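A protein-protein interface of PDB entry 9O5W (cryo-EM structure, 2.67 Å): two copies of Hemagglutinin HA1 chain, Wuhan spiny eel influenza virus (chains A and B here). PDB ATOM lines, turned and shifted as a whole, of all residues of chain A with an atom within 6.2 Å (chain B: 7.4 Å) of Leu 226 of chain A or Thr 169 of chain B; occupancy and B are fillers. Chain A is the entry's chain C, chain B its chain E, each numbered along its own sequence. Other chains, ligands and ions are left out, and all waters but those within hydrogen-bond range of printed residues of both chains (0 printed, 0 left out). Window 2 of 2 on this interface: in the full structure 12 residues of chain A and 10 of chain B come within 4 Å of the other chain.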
ATOM      1  N   TRP A 192      14.441  17.790  31.541  1.00  0.00           N
ATOM      2  CA  TRP A 192      14.799  17.572  30.153  1.00  0.00           C
ATOM      3  C   TRP A 192      15.365  18.867  29.597  1.00  0.00           C
ATOM      4  O   TRP A 192      14.730  19.920  29.711  1.00  0.00           O
ATOM      5  CB  TRP A 192      13.580  17.149  29.338  1.00  0.00           C
ATOM      6  CG  TRP A 192      13.906  16.722  27.943  1.00  0.00           C
ATOM      7  CD1 TRP A 192      13.860  17.497  26.826  1.00  0.00           C
ATOM      8  CD2 TRP A 192      14.323  15.422  27.512  1.00  0.00           C
ATOM      9  NE1 TRP A 192      14.216  16.764  25.724  1.00  0.00           N
ATOM     10  CE2 TRP A 192      14.507  15.486  26.118  1.00  0.00           C
ATOM     11  CE3 TRP A 192      14.553  14.210  28.166  1.00  0.00           C
ATOM     12  CZ2 TRP A 192      14.913  14.386  25.370  1.00  0.00           C
ATOM     13  CZ3 TRP A 192      14.958  13.121  27.423  1.00  0.00           C
ATOM     14  CH2 TRP A 192      15.130  13.214  26.040  1.00  0.00           C
ATOM     15  N   ALA A 193      16.556  18.796  29.006  1.00  0.00           N
ATOM     16  CA  ALA A 193      17.164  19.932  28.339  1.00  0.00           C
ATOM     17  C   ALA A 193      17.270  19.546  26.878  1.00  0.00           C
ATOM     18  O   ALA A 193      17.557  18.392  26.553  1.00  0.00           O
ATOM     19  CB  ALA A 193      18.537  20.263  28.922  1.00  0.00           C
ATOM     20  N   ASP A 194      17.027  20.505  26.001  1.00  0.00           N
ATOM     21  CA  ASP A 194      17.035  20.236  24.578  1.00  0.00           C
ATOM     22  C   ASP A 194      17.348  21.532  23.853  1.00  0.00           C
ATOM     23  O   ASP A 194      17.576  22.572  24.474  1.00  0.00           O
ATOM     24  CB  ASP A 194      15.681  19.649  24.165  1.00  0.00           C
ATOM     25  CG  ASP A 194      15.787  18.703  23.007  1.00  0.00           C
ATOM     26  OD1 ASP A 194      16.567  18.995  22.090  1.00  0.00           O
ATOM     27  OD2 ASP A 194      15.097  17.663  23.020  1.00  0.00           O
ATOM     28  N   LEU A 195      17.374  21.462  22.529  1.00  0.00           N
ATOM     29  CA  LEU A 195      17.618  22.657  21.745  1.00  0.00           C
ATOM     30  C   LEU A 195      16.407  23.559  21.935  1.00  0.00           C
ATOM     31  O   LEU A 195      15.300  23.076  22.188  1.00  0.00           O
ATOM     32  CB  LEU A 195      17.810  22.303  20.272  1.00  0.00           C
ATOM     33  CG  LEU A 195      18.971  21.362  19.930  1.00  0.00           C
ATOM     34  CD1 LEU A 195      18.969  21.055  18.446  1.00  0.00           C
ATOM     35  CD2 LEU A 195      20.314  21.926  20.348  1.00  0.00           C
ATOM     36  N   SER A 196      16.614  24.879  21.867  1.00  0.00           N
ATOM     37  CA  SER A 196      15.485  25.774  22.114  1.00  0.00           C
ATOM     38  C   SER A 196      14.355  25.544  21.116  1.00  0.00           C
ATOM     39  O   SER A 196      13.179  25.703  21.468  1.00  0.00           O
ATOM     40  CB  SER A 196      15.947  27.229  22.067  1.00  0.00           C
ATOM     41  OG  SER A 196      16.382  27.588  20.768  1.00  0.00           O
ATOM     42  N   MET A 199      12.700  22.467  22.626  1.00  0.00           N
ATOM     43  CA  MET A 199      12.001  22.773  23.863  1.00  0.00           C
ATOM     44  C   MET A 199      10.738  23.555  23.550  1.00  0.00           C
ATOM     45  O   MET A 199       9.737  23.422  24.255  1.00  0.00           O
ATOM     46  CB  MET A 199      12.892  23.580  24.807  1.00  0.00           C
ATOM     47  CG  MET A 199      14.055  22.821  25.406  1.00  0.00           C
ATOM     48  SD  MET A 199      13.609  21.388  26.405  1.00  0.00           S
ATOM     49  CE  MET A 199      13.008  22.178  27.893  1.00  0.00           C
ATOM     50  N   VAL A 205       8.552  26.550  25.243  1.00  0.00           N
ATOM     51  CA  VAL A 205       9.514  27.481  25.823  1.00  0.00           C
ATOM     52  C   VAL A 205      10.816  27.400  25.042  1.00  0.00           C
ATOM     53  O   VAL A 205      11.179  26.343  24.517  1.00  0.00           O
ATOM     54  CB  VAL A 205       9.751  27.196  27.326  1.00  0.00           C
ATOM     55  CG1 VAL A 205       8.465  27.391  28.109  1.00  0.00           C
ATOM     56  CG2 VAL A 205      10.291  25.779  27.554  1.00  0.00           C
ATOM     57  N   THR A 206      11.521  28.534  24.969  1.00  0.00           N
ATOM     58  CA  THR A 206      12.814  28.621  24.303  1.00  0.00           C
ATOM     59  C   THR A 206      13.981  28.928  25.231  1.00  0.00           C
ATOM     60  O   THR A 206      15.131  28.759  24.812  1.00  0.00           O
ATOM     61  CB  THR A 206      12.774  29.703  23.211  1.00  0.00           C
ATOM     62  OG1 THR A 206      12.425  30.965  23.794  1.00  0.00           O
ATOM     63  CG2 THR A 206      11.777  29.351  22.123  1.00  0.00           C
ATOM     64  N   THR A 207      13.727  29.364  26.470  1.00  0.00           N
ATOM     65  CA  THR A 207      14.780  29.742  27.401  1.00  0.00           C
ATOM     66  C   THR A 207      14.980  28.674  28.469  1.00  0.00           C
ATOM     67  O   THR A 207      14.129  27.799  28.653  1.00  0.00           O
ATOM     68  CB  THR A 207      14.455  31.081  28.069  1.00  0.00           C
ATOM     69  OG1 THR A 207      13.063  31.130  28.401  1.00  0.00           O
ATOM     70  CG2 THR A 207      14.798  32.235  27.138  1.00  0.00           C
ATOM     71  N   PRO A 208      16.103  28.715  29.193  1.00  0.00           N
ATOM     72  CA  PRO A 208      16.278  27.811  30.336  1.00  0.00           C
ATOM     73  C   PRO A 208      15.176  27.976  31.368  1.00  0.00           C
ATOM     74  O   PRO A 208      14.725  29.087  31.649  1.00  0.00           O
ATOM     75  CB  PRO A 208      17.637  28.228  30.906  1.00  0.00           C
ATOM     76  CG  PRO A 208      18.362  28.789  29.763  1.00  0.00           C
ATOM     77  CD  PRO A 208      17.330  29.495  28.941  1.00  0.00           C
ATOM     78  N   GLN A 209      14.750  26.852  31.937  1.00  0.00           N
ATOM     79  CA  GLN A 209      13.714  26.828  32.956  1.00  0.00           C
ATOM     80  C   GLN A 209      14.386  26.588  34.300  1.00  0.00           C
ATOM     81  O   GLN A 209      15.449  25.969  34.375  1.00  0.00           O
ATOM     82  CB  GLN A 209      12.686  25.733  32.650  1.00  0.00           C
ATOM     83  CG  GLN A 209      12.042  25.837  31.266  1.00  0.00           C
ATOM     84  CD  GLN A 209      11.164  27.059  31.114  1.00  0.00           C
ATOM     85  OE1 GLN A 209      10.163  27.206  31.811  1.00  0.00           O
ATOM     86  NE2 GLN A 209      11.534  27.945  30.201  1.00  0.00           N
ATOM     87  N   PRO A 224      19.045  24.478  33.546  1.00  0.00           N
ATOM     88  CA  PRO A 224      19.801  23.825  32.466  1.00  0.00           C
ATOM     89  C   PRO A 224      19.938  24.653  31.196  1.00  0.00           C
ATOM     90  O   PRO A 224      18.969  25.233  30.706  1.00  0.00           O
ATOM     91  CB  PRO A 224      18.986  22.558  32.204  1.00  0.00           C
ATOM     92  CG  PRO A 224      18.357  22.256  33.482  1.00  0.00           C
ATOM     93  CD  PRO A 224      17.999  23.577  34.070  1.00  0.00           C
ATOM     94  N   PHE A 225      21.150  24.688  30.645  1.00  0.00           N
ATOM     95  CA  PHE A 225      21.365  25.425  29.412  1.00  0.00           C
ATOM     96  C   PHE A 225      20.766  24.619  28.266  1.00  0.00           C
ATOM     97  O   PHE A 225      20.797  23.386  28.272  1.00  0.00           O
ATOM     98  CB  PHE A 225      22.856  25.669  29.164  1.00  0.00           C
ATOM     99  CG  PHE A 225      23.492  26.639  30.129  1.00  0.00           C
ATOM    100  CD1 PHE A 225      22.978  27.909  30.312  1.00  0.00           C
ATOM    101  CD2 PHE A 225      24.623  26.278  30.838  1.00  0.00           C
ATOM    102  CE1 PHE A 225      23.565  28.786  31.199  1.00  0.00           C
ATOM    103  CE2 PHE A 225      25.213  27.156  31.724  1.00  0.00           C
ATOM    104  CZ  PHE A 225      24.687  28.411  31.899  1.00  0.00           C
ATOM    105  N   LEU A 226      20.219  25.319  27.275  1.00  0.00           N
ATOM    106  CA  LEU A 226      19.582  24.675  26.131  1.00  0.00           C
ATOM    107  C   LEU A 226      20.495  24.716  24.910  1.00  0.00           C
ATOM    108  O   LEU A 226      20.655  25.765  24.279  1.00  0.00           O
ATOM    109  CB  LEU A 226      18.245  25.352  25.837  1.00  0.00           C
ATOM    110  CG  LEU A 226      17.236  25.379  26.991  1.00  0.00           C
ATOM    111  CD1 LEU A 226      15.962  26.068  26.547  1.00  0.00           C
ATOM    112  CD2 LEU A 226      16.946  23.999  27.583  1.00  0.00           C
ATOM    113  N   GLY A 227      21.049  23.559  24.561  1.00  0.00           N
ATOM    114  CA  GLY A 227      21.971  23.404  23.452  1.00  0.00           C
ATOM    115  C   GLY A 227      23.415  23.379  23.907  1.00  0.00           C
ATOM    116  O   GLY A 227      23.742  23.570  25.082  1.00  0.00           O
ATOM    117  N   ASN A 228      24.296  23.161  22.930  1.00  0.00           N
ATOM    118  CA  ASN A 228      25.731  23.038  23.177  1.00  0.00           C
ATOM    119  C   ASN A 228      26.005  21.966  24.228  1.00  0.00           C
ATOM    120  O   ASN A 228      26.763  22.165  25.179  1.00  0.00           O
ATOM    121  CB  ASN A 228      26.329  24.382  23.593  1.00  0.00           C
ATOM    122  CG  ASN A 228      27.828  24.436  23.401  1.00  0.00           C
ATOM    123  OD1 ASN A 228      28.370  23.851  22.464  1.00  0.00           O
ATOM    124  ND2 ASN A 228      28.509  25.136  24.294  1.00  0.00           N
ATOM    125  N   PHE A 229      25.376  20.819  24.050  1.00  0.00           N
ATOM    126  CA  PHE A 229      25.508  19.740  25.011  1.00  0.00           C
ATOM    127  C   PHE A 229      26.848  19.009  24.877  1.00  0.00           C
ATOM    128  O   PHE A 229      27.446  18.987  23.798  1.00  0.00           O
ATOM    129  CB  PHE A 229      24.378  18.734  24.826  1.00  0.00           C
ATOM    130  CG  PHE A 229      23.020  19.276  25.157  1.00  0.00           C
ATOM    131  CD1 PHE A 229      22.716  19.702  26.436  1.00  0.00           C
ATOM    132  CD2 PHE A 229      22.047  19.363  24.182  1.00  0.00           C
ATOM    133  CE1 PHE A 229      21.468  20.201  26.733  1.00  0.00           C
ATOM    134  CE2 PHE A 229      20.803  19.865  24.475  1.00  0.00           C
ATOM    135  CZ  PHE A 229      20.513  20.280  25.753  1.00  0.00           C
ATOM    136  N   GLY B 166      28.973  38.775  22.430  1.00  0.00           N
ATOM    137  CA  GLY B 166      27.533  38.608  22.413  1.00  0.00           C
ATOM    138  C   GLY B 166      27.104  37.467  23.305  1.00  0.00           C
ATOM    139  O   GLY B 166      27.937  36.655  23.716  1.00  0.00           O
ATOM    140  N   ALA B 167      25.816  37.396  23.624  1.00  0.00           N
ATOM    141  CA  ALA B 167      25.335  36.339  24.496  1.00  0.00           C
ATOM    142  C   ALA B 167      25.488  34.985  23.820  1.00  0.00           C
ATOM    143  O   ALA B 167      25.347  34.855  22.602  1.00  0.00           O
ATOM    144  CB  ALA B 167      23.871  36.573  24.862  1.00  0.00           C
ATOM    145  N   ILE B 168      25.788  33.972  24.631  1.00  0.00           N
ATOM    146  CA  ILE B 168      25.925  32.598  24.174  1.00  0.00           C
ATOM    147  C   ILE B 168      25.055  31.686  25.028  1.00  0.00           C
ATOM    148  O   ILE B 168      24.596  32.056  26.110  1.00  0.00           O
ATOM    149  CB  ILE B 168      27.410  32.143  24.190  1.00  0.00           C
ATOM    150  CG1 ILE B 168      27.994  32.158  25.620  1.00  0.00           C
ATOM    151  CG2 ILE B 168      28.229  33.013  23.233  1.00  0.00           C
ATOM    152  CD1 ILE B 168      29.377  31.547  25.756  1.00  0.00           C
ATOM    153  N   THR B 169      24.827  30.478  24.512  1.00  0.00           N
ATOM    154  CA  THR B 169      24.081  29.476  25.265  1.00  0.00           C
ATOM    155  C   THR B 169      24.815  29.108  26.544  1.00  0.00           C
ATOM    156  O   THR B 169      24.201  28.967  27.607  1.00  0.00           O
ATOM    157  CB  THR B 169      23.860  28.239  24.389  1.00  0.00           C
ATOM    158  OG1 THR B 169      23.066  28.593  23.250  1.00  0.00           O
ATOM    159  CG2 THR B 169      23.168  27.101  25.148  1.00  0.00           C
ATOM    160  N   GLY B 170      26.129  28.952  26.453  1.00  0.00           N
ATOM    161  CA  GLY B 170      26.970  28.544  27.564  1.00  0.00           C
ATOM    162  C   GLY B 170      27.875  27.441  27.054  1.00  0.00           C
ATOM    163  O   GLY B 170      27.546  26.723  26.107  1.00  0.00           O
ATOM    164  N   GLU B 171      29.031  27.306  27.692  1.00  0.00           N
ATOM    165  CA  GLU B 171      30.046  26.331  27.331  1.00  0.00           C
ATOM    166  C   GLU B 171      30.278  25.432  28.534  1.00  0.00           C
ATOM    167  O   GLU B 171      30.033  25.836  29.666  1.00  0.00           O
ATOM    168  CB  GLU B 171      31.351  27.019  26.926  1.00  0.00           C
ATOM    169  CG  GLU B 171      31.216  27.944  25.727  1.00  0.00           C
ATOM    170  CD  GLU B 171      30.982  27.205  24.432  1.00  0.00           C
ATOM    171  OE1 GLU B 171      31.152  25.969  24.409  1.00  0.00           O
ATOM    172  OE2 GLU B 171      30.622  27.860  23.430  1.00  0.00           O
ATOM    173  N   THR B 210      25.400  33.438  33.839  1.00  0.00           N
ATOM    174  CA  THR B 210      25.296  32.303  34.751  1.00  0.00           C
ATOM    175  C   THR B 210      26.542  31.430  34.715  1.00  0.00           C
ATOM    176  O   THR B 210      27.003  31.040  33.637  1.00  0.00           O
ATOM    177  CB  THR B 210      24.056  31.470  34.403  1.00  0.00           C
ATOM    178  OG1 THR B 210      22.887  32.285  34.536  1.00  0.00           O
ATOM    179  CG2 THR B 210      23.896  30.256  35.332  1.00  0.00           C
ATOM    180  N   TYR B 261      29.840  27.567  31.900  1.00  0.00           N
ATOM    181  CA  TYR B 261      30.117  28.994  32.007  1.00  0.00           C
ATOM    182  C   TYR B 261      29.612  29.749  30.782  1.00  0.00           C
ATOM    183  O   TYR B 261      29.718  29.256  29.660  1.00  0.00           O
ATOM    184  CB  TYR B 261      31.632  29.189  32.203  1.00  0.00           C
ATOM    185  CG  TYR B 261      32.515  28.885  30.991  1.00  0.00           C
ATOM    186  CD1 TYR B 261      32.645  29.786  29.936  1.00  0.00           C
ATOM    187  CD2 TYR B 261      33.260  27.718  30.937  1.00  0.00           C
ATOM    188  CE1 TYR B 261      33.455  29.521  28.867  1.00  0.00           C
ATOM    189  CE2 TYR B 261      34.074  27.445  29.861  1.00  0.00           C
ATOM    190  CZ  TYR B 261      34.159  28.348  28.828  1.00  0.00           C
ATOM    191  OH  TYR B 261      34.954  28.095  27.741  1.00  0.00           O
ATOM    192  N   GLN B 262      29.060  30.945  31.008  1.00  0.00           N
ATOM    193  CA  GLN B 262      28.673  31.854  29.929  1.00  0.00           C
ATOM    194  C   GLN B 262      29.786  32.889  29.742  1.00  0.00           C
ATOM    195  O   GLN B 262      30.936  32.618  30.093  1.00  0.00           O
ATOM    196  CB  GLN B 262      27.311  32.498  30.209  1.00  0.00           C
ATOM    197  CG  GLN B 262      26.144  31.542  30.177  1.00  0.00           C
ATOM    198  CD  GLN B 262      24.844  32.232  30.524  1.00  0.00           C
ATOM    199  OE1 GLN B 262      24.833  33.250  31.212  1.00  0.00           O
ATOM    200  NE2 GLN B 262      23.742  31.701  30.020  1.00  0.00           N
ATOM    201  N   ARG B 263      29.479  34.066  29.197  1.00  0.00           N
ATOM    202  CA  ARG B 263      30.503  35.084  29.004  1.00  0.00           C
ATOM    203  C   ARG B 263      30.937  35.667  30.340  1.00  0.00           C
ATOM    204  O   ARG B 263      30.187  35.665  31.314  1.00  0.00           O
ATOM    205  CB  ARG B 263      29.983  36.211  28.113  1.00  0.00           C
ATOM    206  CG  ARG B 263      29.667  35.796  26.693  1.00  0.00           C
ATOM    207  CD  ARG B 263      30.881  35.887  25.791  1.00  0.00           C
ATOM    208  NE  ARG B 263      30.493  35.759  24.391  1.00  0.00           N
ATOM    209  CZ  ARG B 263      31.256  35.277  23.419  1.00  0.00           C
ATOM    210  NH1 ARG B 263      32.493  34.860  23.641  1.00  0.00           N
ATOM    211  NH2 ARG B 263      30.763  35.205  22.187  1.00  0.00           N
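ND2 of Asn 228 of chain A is in hydrogen-bond range of OE1 of Glu 171 of chain B (2.8 Å). The side-chain amide nitrogen (ND2) of Asn 228 of chain A lies within hydrogen-bond range of the backbone carbonyl oxygen (O) of Gly 170 of chain B (2.6 Å).
Among the printed residues, merely in contact across the chains: Phe 225 of chain A with Thr 169 of chain B (3.2 Å), Phe 225 of chain A with Thr 210 of chain B (3.9 Å), Phe 225 of chain A with Gln 262 of chain B (3.1 Å), Leu 226 of chain A with Thr 169 of chain B (3.0 Å) and Gly 227 of chain A with Thr 169 of chain B (3.6 Å).
Thr 169 of chain B touches just these residues of chain A: Phe 225, Leu 226 and Gly 227. Of the printed residues of chain B, Phe 225 of chain A touches Thr 169 (3.2 Å), Thr 210 (3.9 Å) and Gln 262 (3.1 Å). Of the printed residues of chain B, Asn 228 of chain A touches Gly 170 and Glu 171. Printed residues of chain A within 4 Å of Thr 210 of chain B: Phe 225 (3.9 Å). Of the printed residues of chain A, Gln 262 of chain B touches Phe 225 (3.1 Å). Of the printed residues of chain A, Glu 171 of chain B touches Asn 228. The nearest residue of chain B that does not touch Leu 226 of chain A is Gly 170 of chain B (6.7 Å).
The backbone carbonyl oxygen of Glu 171 of chain B sits at hydrogen-bond distance from the backbone NH of Tyr 261 of chain B, at 2.8 Å. N of Thr 210 of chain B lies within hydrogen-bond range of OE1 of Gln 262 of chain B (2.7 Å).
No position is printed for both chains. Of the 7 pairs that touch across the chains among the printed residues, none has its exchanged pair printed and touching as well.
Printed residues of chain A that touch a printed residue of chain B: Phe 225, Leu 226, Gly 227 and Asn 228. Hydrophobic or aromatic side chains of chain A that line the printed part of chain B: Phe 225. Printed residues of chain B that touch a printed residue of chain A: Thr 169, Gly 170, Glu 171, Thr 210 and Gln 262.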
